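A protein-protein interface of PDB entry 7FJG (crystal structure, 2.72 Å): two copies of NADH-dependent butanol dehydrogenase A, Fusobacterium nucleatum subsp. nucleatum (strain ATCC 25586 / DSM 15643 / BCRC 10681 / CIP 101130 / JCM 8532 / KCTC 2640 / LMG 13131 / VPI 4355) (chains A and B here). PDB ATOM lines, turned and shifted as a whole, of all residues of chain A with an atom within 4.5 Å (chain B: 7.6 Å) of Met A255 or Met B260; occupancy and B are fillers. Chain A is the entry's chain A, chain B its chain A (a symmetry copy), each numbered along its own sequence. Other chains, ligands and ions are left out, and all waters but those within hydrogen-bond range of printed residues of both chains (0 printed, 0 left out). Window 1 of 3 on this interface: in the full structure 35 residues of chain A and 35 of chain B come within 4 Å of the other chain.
NE1 of Trp A251 sits at hydrogen-bond distance from O of Met B260, 3.3 Å away.
The indole nitrogen (NE1) of Trp A251 is in hydrogen-bond range of the side-chain sulfur (SG) of Cys B263 (2.9 Å).
The side-chain sulfur (SD) of Met B260 lies within hydrogen-bond range of the side-chain amide nitrogen (ND2) of Asn A258 (3.6 Å).
O of Ile B261 lies within hydrogen-bond range of OG of Ser B218 (2.7 Å).
The side-chain amide oxygen of Asn B258 sits close to the backbone NH of Met B260.
SG of Cys B263 is in hydrogen-bond range of O of Met B260 (3.4 Å).
Among the printed residues, pairs that only touch across the chains: Trp A251 with Phe B4 (3.5 Å), Trp A251 with Leu B217 (3.4 Å), Ala A252 with Leu B217 (3.4 Å), Met A255 with Leu B221 (3.6 Å), Met A255 with Met B260 (3.9 Å), Met A255 with Ile B261 (3.8 Å) and Ile A261 with Met B255 (3.8 Å).
Met A255 touches three residues of chain B.
Of chain A, only Trp A251 (3.3 Å), Met A255 (3.9 Å) and Asn A258 (3.6 Å) come within 4 Å of Met B260.
Printed residues of chain A within 4 Å of Cys B263: Trp A251 (2.9 Å).
Printed residues of chain A within 4 Å of Ile B261: Met A255 (3.8 Å).
Gly B259 touches none of the printed residues of chain A.
The nearest residue of chain B that does not touch Met A255 is Leu B217 (4.6 Å).
The nearest residue of chain A that does not touch Met B260 is Thr A254 (4.3 Å).
Hydrophobic or aromatic side chains of chain B that line the printed part of chain A: Phe B4, Leu B217, Leu B221, Met B255, Met B260 and Ile B261.
Hydrophobic or aromatic side chains of chain A that line the printed part of chain B: Trp A251, Met A255 and Ile A261.
Among the printed residues, 10 pairs touch across the chains.
Among the printed residues, no Asp or Glu carboxylate lies within 4 Å of a Lys or Arg side-chain nitrogen of the other chain.
Met A255 touches Ile B261, and with the chains exchanged Ile A261 touches Met B255.
Positions printed for both chains: 255, 256, 257, 258 and 261.
Of the 10 pairs that touch across the chains among the printed residues, 2 have their exchanged pair printed and touching as well.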
ATOM      1  N   TRP A 251      37.899  18.814  19.389  1.00  0.00           N
ATOM      2  CA  TRP A 251      36.487  18.592  19.056  1.00  0.00           C
ATOM      3  C   TRP A 251      35.861  19.887  18.538  1.00  0.00           C
ATOM      4  O   TRP A 251      35.072  19.854  17.586  1.00  0.00           O
ATOM      5  CB  TRP A 251      35.701  17.983  20.250  1.00  0.00           C
ATOM      6  CG  TRP A 251      34.293  17.431  19.843  1.00  0.00           C
ATOM      7  CD1 TRP A 251      33.081  17.736  20.420  1.00  0.00           C
ATOM      8  CD2 TRP A 251      33.992  16.517  18.775  1.00  0.00           C
ATOM      9  NE1 TRP A 251      32.048  17.087  19.752  1.00  0.00           N
ATOM     10  CE2 TRP A 251      32.588  16.340  18.743  1.00  0.00           C
ATOM     11  CE3 TRP A 251      34.773  15.806  17.873  1.00  0.00           C
ATOM     12  CZ2 TRP A 251      31.974  15.501  17.839  1.00  0.00           C
ATOM     13  CZ3 TRP A 251      34.157  15.005  16.958  1.00  0.00           C
ATOM     14  CH2 TRP A 251      32.777  14.851  16.939  1.00  0.00           C
ATOM     15  N   ALA A 252      36.290  21.049  19.072  1.00  0.00           N
ATOM     16  CA  ALA A 252      35.777  22.333  18.593  1.00  0.00           C
ATOM     17  C   ALA A 252      36.139  22.559  17.129  1.00  0.00           C
ATOM     18  O   ALA A 252      35.302  23.016  16.325  1.00  0.00           O
ATOM     19  CB  ALA A 252      36.324  23.478  19.444  1.00  0.00           C
ATOM     20  N   ALA A 253      37.396  22.251  16.763  1.00  0.00           N
ATOM     21  CA  ALA A 253      37.827  22.437  15.381  1.00  0.00           C
ATOM     22  C   ALA A 253      37.009  21.556  14.468  1.00  0.00           C
ATOM     23  O   ALA A 253      36.566  21.990  13.397  1.00  0.00           O
ATOM     24  CB  ALA A 253      39.305  22.118  15.219  1.00  0.00           C
ATOM     25  N   THR A 254      36.744  20.332  14.906  1.00  0.00           N
ATOM     26  CA  THR A 254      35.921  19.452  14.097  1.00  0.00           C
ATOM     27  C   THR A 254      34.544  20.059  13.865  1.00  0.00           C
ATOM     28  O   THR A 254      34.078  20.157  12.716  1.00  0.00           O
ATOM     29  CB  THR A 254      35.805  18.088  14.766  1.00  0.00           C
ATOM     30  OG1 THR A 254      37.084  17.447  14.698  1.00  0.00           O
ATOM     31  CG2 THR A 254      34.690  17.257  14.062  1.00  0.00           C
ATOM     32  N   MET A 255      33.882  20.474  14.958  1.00  0.00           N
ATOM     33  CA  MET A 255      32.566  21.077  14.832  1.00  0.00           C
ATOM     34  C   MET A 255      32.612  22.352  14.007  1.00  0.00           C
ATOM     35  O   MET A 255      31.753  22.561  13.153  1.00  0.00           O
ATOM     36  CB  MET A 255      31.973  21.381  16.197  1.00  0.00           C
ATOM     37  CG  MET A 255      31.608  20.165  17.052  1.00  0.00           C
ATOM     38  SD  MET A 255      30.164  19.307  16.487  1.00  0.00           S
ATOM     39  CE  MET A 255      28.816  20.353  17.019  1.00  0.00           C
ATOM     40  N   ALA A 256      33.590  23.224  14.246  1.00  0.00           N
ATOM     41  CA  ALA A 256      33.744  24.374  13.365  1.00  0.00           C
ATOM     42  C   ALA A 256      33.674  23.977  11.883  1.00  0.00           C
ATOM     43  O   ALA A 256      33.139  24.721  11.062  1.00  0.00           O
ATOM     44  CB  ALA A 256      35.062  25.090  13.690  1.00  0.00           C
ATOM     45  N   HIS A 257      34.158  22.800  11.527  1.00  0.00           N
ATOM     46  CA  HIS A 257      34.131  22.340  10.145  1.00  0.00           C
ATOM     47  C   HIS A 257      32.826  21.642   9.772  1.00  0.00           C
ATOM     48  O   HIS A 257      32.747  20.979   8.730  1.00  0.00           O
ATOM     49  CB  HIS A 257      35.320  21.417   9.903  1.00  0.00           C
ATOM     50  CG  HIS A 257      36.631  22.122   9.989  1.00  0.00           C
ATOM     51  ND1 HIS A 257      36.843  23.350   9.401  1.00  0.00           N
ATOM     52  CD2 HIS A 257      37.797  21.780  10.591  1.00  0.00           C
ATOM     53  CE1 HIS A 257      38.088  23.732   9.624  1.00  0.00           C
ATOM     54  NE2 HIS A 257      38.685  22.801  10.351  1.00  0.00           N
ATOM     55  N   ASN A 258      31.794  21.804  10.578  1.00  0.00           N
ATOM     56  CA  ASN A 258      30.548  21.072  10.408  1.00  0.00           C
ATOM     57  C   ASN A 258      29.457  22.043   9.995  1.00  0.00           C
ATOM     58  O   ASN A 258      29.236  23.070  10.651  1.00  0.00           O
ATOM     59  CB  ASN A 258      30.158  20.336  11.701  1.00  0.00           C
ATOM     60  CG  ASN A 258      29.227  19.170  11.447  1.00  0.00           C
ATOM     61  OD1 ASN A 258      28.061  19.220  11.822  1.00  0.00           O
ATOM     62  ND2 ASN A 258      29.736  18.119  10.779  1.00  0.00           N
ATOM     63  N   ILE A 261      26.105  23.222  12.296  1.00  0.00           N
ATOM     64  CA  ILE A 261      25.917  24.379  13.151  1.00  0.00           C
ATOM     65  C   ILE A 261      25.849  25.648  12.321  1.00  0.00           C
ATOM     66  O   ILE A 261      25.022  26.515  12.591  1.00  0.00           O
ATOM     67  CB  ILE A 261      26.990  24.448  14.244  1.00  0.00           C
ATOM     68  CG1 ILE A 261      28.396  24.418  13.665  1.00  0.00           C
ATOM     69  CG2 ILE A 261      26.762  23.320  15.253  1.00  0.00           C
ATOM     70  CD1 ILE A 261      29.385  25.255  14.525  1.00  0.00           C
ATOM     71  N   PHE B   4      34.573   7.837  21.397  1.00  0.00           N
ATOM     72  CA  PHE B   4      33.299   7.698  20.700  1.00  0.00           C
ATOM     73  C   PHE B   4      33.543   7.699  19.195  1.00  0.00           C
ATOM     74  O   PHE B   4      34.564   8.213  18.711  1.00  0.00           O
ATOM     75  CB  PHE B   4      32.285   8.804  21.125  1.00  0.00           C
ATOM     76  CG  PHE B   4      32.605  10.164  20.603  1.00  0.00           C
ATOM     77  CD1 PHE B   4      32.150  10.573  19.365  1.00  0.00           C
ATOM     78  CD2 PHE B   4      33.393  11.032  21.344  1.00  0.00           C
ATOM     79  CE1 PHE B   4      32.477  11.838  18.858  1.00  0.00           C
ATOM     80  CE2 PHE B   4      33.730  12.290  20.850  1.00  0.00           C
ATOM     81  CZ  PHE B   4      33.267  12.697  19.598  1.00  0.00           C
ATOM     82  N   ASN B   5      32.607   7.061  18.476  1.00  0.00           N
ATOM     83  CA  ASN B   5      32.523   7.092  17.023  1.00  0.00           C
ATOM     84  C   ASN B   5      31.258   7.815  16.551  1.00  0.00           C
ATOM     85  O   ASN B   5      30.262   7.919  17.271  1.00  0.00           O
ATOM     86  CB  ASN B   5      32.568   5.668  16.448  1.00  0.00           C
ATOM     87  CG  ASN B   5      33.842   4.952  16.808  1.00  0.00           C
ATOM     88  OD1 ASN B   5      34.774   4.880  16.016  1.00  0.00           O
ATOM     89  ND2 ASN B   5      33.901   4.434  18.017  1.00  0.00           N
ATOM     90  N   TYR B   6      31.314   8.360  15.335  1.00  0.00           N
ATOM     91  CA  TYR B   6      30.129   9.001  14.776  1.00  0.00           C
ATOM     92  C   TYR B   6      30.056   8.847  13.267  1.00  0.00           C
ATOM     93  O   TYR B   6      30.973   9.257  12.542  1.00  0.00           O
ATOM     94  CB  TYR B   6      30.077  10.478  15.134  1.00  0.00           C
ATOM     95  CG  TYR B   6      29.029  11.247  14.349  1.00  0.00           C
ATOM     96  CD1 TYR B   6      27.684  11.232  14.741  1.00  0.00           C
ATOM     97  CD2 TYR B   6      29.380  11.987  13.220  1.00  0.00           C
ATOM     98  CE1 TYR B   6      26.725  11.920  14.033  1.00  0.00           C
ATOM     99  CE2 TYR B   6      28.429  12.692  12.512  1.00  0.00           C
ATOM    100  CZ  TYR B   6      27.100  12.663  12.917  1.00  0.00           C
ATOM    101  OH  TYR B   6      26.158  13.380  12.183  1.00  0.00           O
ATOM    102  N   LYS B   7      28.927   8.310  12.806  1.00  0.00           N
ATOM    103  CA  LYS B   7      28.587   8.277  11.393  1.00  0.00           C
ATOM    104  C   LYS B   7      27.154   8.750  11.216  1.00  0.00           C
ATOM    105  O   LYS B   7      26.285   8.485  12.060  1.00  0.00           O
ATOM    106  CB  LYS B   7      28.729   6.883  10.835  1.00  0.00           C
ATOM    107  CG  LYS B   7      29.125   6.808   9.392  1.00  0.00           C
ATOM    108  CD  LYS B   7      29.662   5.385   9.075  1.00  0.00           C
ATOM    109  CE  LYS B   7      29.477   5.000   7.599  1.00  0.00           C
ATOM    110  NZ  LYS B   7      29.903   6.123   6.705  1.00  0.00           N
ATOM    111  N   ASN B   8      26.920   9.463  10.124  1.00  0.00           N
ATOM    112  CA  ASN B   8      25.559   9.712   9.669  1.00  0.00           C
ATOM    113  C   ASN B   8      25.585  10.267   8.254  1.00  0.00           C
ATOM    114  O   ASN B   8      25.958  11.424   8.025  1.00  0.00           O
ATOM    115  CB  ASN B   8      24.823  10.663  10.605  1.00  0.00           C
ATOM    116  CG  ASN B   8      23.343  10.690  10.332  1.00  0.00           C
ATOM    117  OD1 ASN B   8      22.908  11.102   9.250  1.00  0.00           O
ATOM    118  ND2 ASN B   8      22.554  10.226  11.289  1.00  0.00           N
ATOM    119  N   LEU B 217      32.567  21.246  25.849  1.00  0.00           N
ATOM    120  CA  LEU B 217      32.038  21.555  24.533  1.00  0.00           C
ATOM    121  C   LEU B 217      30.661  20.944  24.340  1.00  0.00           C
ATOM    122  O   LEU B 217      29.688  21.644  24.005  1.00  0.00           O
ATOM    123  CB  LEU B 217      32.968  21.052  23.450  1.00  0.00           C
ATOM    124  CG  LEU B 217      32.432  21.233  22.046  1.00  0.00           C
ATOM    125  CD1 LEU B 217      31.962  22.649  21.936  1.00  0.00           C
ATOM    126  CD2 LEU B 217      33.605  20.979  21.102  1.00  0.00           C
ATOM    127  N   SER B 218      30.562  19.629  24.526  1.00  0.00           N
ATOM    128  CA  SER B 218      29.273  18.982  24.332  1.00  0.00           C
ATOM    129  C   SER B 218      28.215  19.551  25.286  1.00  0.00           C
ATOM    130  O   SER B 218      27.060  19.784  24.891  1.00  0.00           O
ATOM    131  CB  SER B 218      29.447  17.480  24.488  1.00  0.00           C
ATOM    132  OG  SER B 218      28.250  16.877  24.928  1.00  0.00           O
ATOM    133  N   LEU B 221      26.861  22.654  23.590  1.00  0.00           N
ATOM    134  CA  LEU B 221      25.997  22.462  22.441  1.00  0.00           C
ATOM    135  C   LEU B 221      24.628  22.000  22.894  1.00  0.00           C
ATOM    136  O   LEU B 221      23.617  22.551  22.464  1.00  0.00           O
ATOM    137  CB  LEU B 221      26.623  21.461  21.482  1.00  0.00           C
ATOM    138  CG  LEU B 221      28.055  21.854  21.086  1.00  0.00           C
ATOM    139  CD1 LEU B 221      28.984  20.743  20.607  1.00  0.00           C
ATOM    140  CD2 LEU B 221      28.000  22.898  19.964  1.00  0.00           C
ATOM    141  N   ILE B 222      24.578  21.029  23.820  1.00  0.00           N
ATOM    142  CA  ILE B 222      23.293  20.556  24.333  1.00  0.00           C
ATOM    143  C   ILE B 222      22.565  21.680  25.047  1.00  0.00           C
ATOM    144  O   ILE B 222      21.345  21.843  24.906  1.00  0.00           O
ATOM    145  CB  ILE B 222      23.472  19.336  25.253  1.00  0.00           C
ATOM    146  CG1 ILE B 222      24.144  18.213  24.427  1.00  0.00           C
ATOM    147  CG2 ILE B 222      22.075  19.011  25.901  1.00  0.00           C
ATOM    148  CD1 ILE B 222      24.394  16.960  25.201  1.00  0.00           C
ATOM    149  N   MET B 255      19.030  18.329  15.435  1.00  0.00           N
ATOM    150  CA  MET B 255      20.278  18.332  16.179  1.00  0.00           C
ATOM    151  C   MET B 255      20.186  17.474  17.430  1.00  0.00           C
ATOM    152  O   MET B 255      21.105  16.713  17.721  1.00  0.00           O
ATOM    153  CB  MET B 255      20.679  19.745  16.565  1.00  0.00           C
ATOM    154  CG  MET B 255      21.077  20.665  15.409  1.00  0.00           C
ATOM    155  SD  MET B 255      22.660  20.283  14.709  1.00  0.00           S
ATOM    156  CE  MET B 255      23.819  20.931  15.906  1.00  0.00           C
ATOM    157  N   ALA B 256      19.098  17.583  18.191  1.00  0.00           N
ATOM    158  CA  ALA B 256      18.918  16.661  19.305  1.00  0.00           C
ATOM    159  C   ALA B 256      19.195  15.207  18.898  1.00  0.00           C
ATOM    160  O   ALA B 256      19.733  14.429  19.685  1.00  0.00           O
ATOM    161  CB  ALA B 256      17.502  16.823  19.875  1.00  0.00           C
ATOM    162  N   HIS B 257      18.884  14.830  17.670  1.00  0.00           N
ATOM    163  CA  HIS B 257      19.114  13.471  17.197  1.00  0.00           C
ATOM    164  C   HIS B 257      20.521  13.260  16.643  1.00  0.00           C
ATOM    165  O   HIS B 257      20.787  12.251  15.979  1.00  0.00           O
ATOM    166  CB  HIS B 257      18.067  13.125  16.145  1.00  0.00           C
ATOM    167  CG  HIS B 257      16.686  13.050  16.701  1.00  0.00           C
ATOM    168  ND1 HIS B 257      16.408  12.410  17.890  1.00  0.00           N
ATOM    169  CD2 HIS B 257      15.505  13.530  16.240  1.00  0.00           C
ATOM    170  CE1 HIS B 257      15.112  12.487  18.134  1.00  0.00           C
ATOM    171  NE2 HIS B 257      14.542  13.168  17.152  1.00  0.00           N
ATOM    172  N   ASN B 258      21.433  14.169  16.930  1.00  0.00           N
ATOM    173  CA  ASN B 258      22.762  14.154  16.338  1.00  0.00           C
ATOM    174  C   ASN B 258      23.780  13.838  17.418  1.00  0.00           C
ATOM    175  O   ASN B 258      23.814  14.488  18.472  1.00  0.00           O
ATOM    176  CB  ASN B 258      23.085  15.501  15.668  1.00  0.00           C
ATOM    177  CG  ASN B 258      24.159  15.379  14.608  1.00  0.00           C
ATOM    178  OD1 ASN B 258      25.265  15.878  14.793  1.00  0.00           O
ATOM    179  ND2 ASN B 258      23.845  14.688  13.499  1.00  0.00           N
ATOM    180  N   GLY B 259      24.580  12.822  17.169  1.00  0.00           N
ATOM    181  CA  GLY B 259      25.604  12.407  18.094  1.00  0.00           C
ATOM    182  C   GLY B 259      26.890  13.181  17.953  1.00  0.00           C
ATOM    183  O   GLY B 259      27.938  12.757  18.471  1.00  0.00           O
ATOM    184  N   MET B 260      26.853  14.303  17.246  1.00  0.00           N
ATOM    185  CA  MET B 260      27.987  15.196  17.348  1.00  0.00           C
ATOM    186  C   MET B 260      27.900  16.017  18.619  1.00  0.00           C
ATOM    187  O   MET B 260      28.909  16.222  19.301  1.00  0.00           O
ATOM    188  CB  MET B 260      28.064  16.053  16.104  1.00  0.00           C
ATOM    189  CG  MET B 260      28.275  15.138  14.929  1.00  0.00           C
ATOM    190  SD  MET B 260      28.928  16.085  13.584  1.00  0.00           S
ATOM    191  CE  MET B 260      30.653  15.889  13.912  1.00  0.00           C
ATOM    192  N   ILE B 261      26.708  16.459  18.993  1.00  0.00           N
ATOM    193  CA  ILE B 261      26.674  17.299  20.175  1.00  0.00           C
ATOM    194  C   ILE B 261      26.694  16.449  21.432  1.00  0.00           C
ATOM    195  O   ILE B 261      27.387  16.786  22.389  1.00  0.00           O
ATOM    196  CB  ILE B 261      25.485  18.267  20.140  1.00  0.00           C
ATOM    197  CG1 ILE B 261      24.163  17.539  19.946  1.00  0.00           C
ATOM    198  CG2 ILE B 261      25.720  19.323  19.057  1.00  0.00           C
ATOM    199  CD1 ILE B 261      23.000  18.266  20.680  1.00  0.00           C
ATOM    200  N   ALA B 262      25.987  15.327  21.458  1.00  0.00           N
ATOM    201  CA  ALA B 262      26.115  14.353  22.545  1.00  0.00           C
ATOM    202  C   ALA B 262      27.163  13.369  22.082  1.00  0.00           C
ATOM    203  O   ALA B 262      26.884  12.553  21.198  1.00  0.00           O
ATOM    204  CB  ALA B 262      24.796  13.655  22.832  1.00  0.00           C
ATOM    205  N   CYS B 263      28.384  13.454  22.625  1.00  0.00           N
ATOM    206  CA  CYS B 263      29.489  12.700  22.019  1.00  0.00           C
ATOM    207  C   CYS B 263      30.323  12.033  23.097  1.00  0.00           C
ATOM    208  O   CYS B 263      31.251  12.647  23.633  1.00  0.00           O
ATOM    209  CB  CYS B 263      30.367  13.568  21.115  1.00  0.00           C
ATOM    210  SG  CYS B 263      31.028  15.214  21.723  1.00  0.00           S
ATOM    211  N   GLY B 264      30.019  10.763  23.363  1.00  0.00           N
ATOM    212  CA  GLY B 264      30.717  10.075  24.418  1.00  0.00           C
ATOM    213  C   GLY B 264      30.169  10.501  25.761  1.00  0.00           C
ATOM    214  O   GLY B 264      30.896  10.931  26.665  1.00  0.00           O
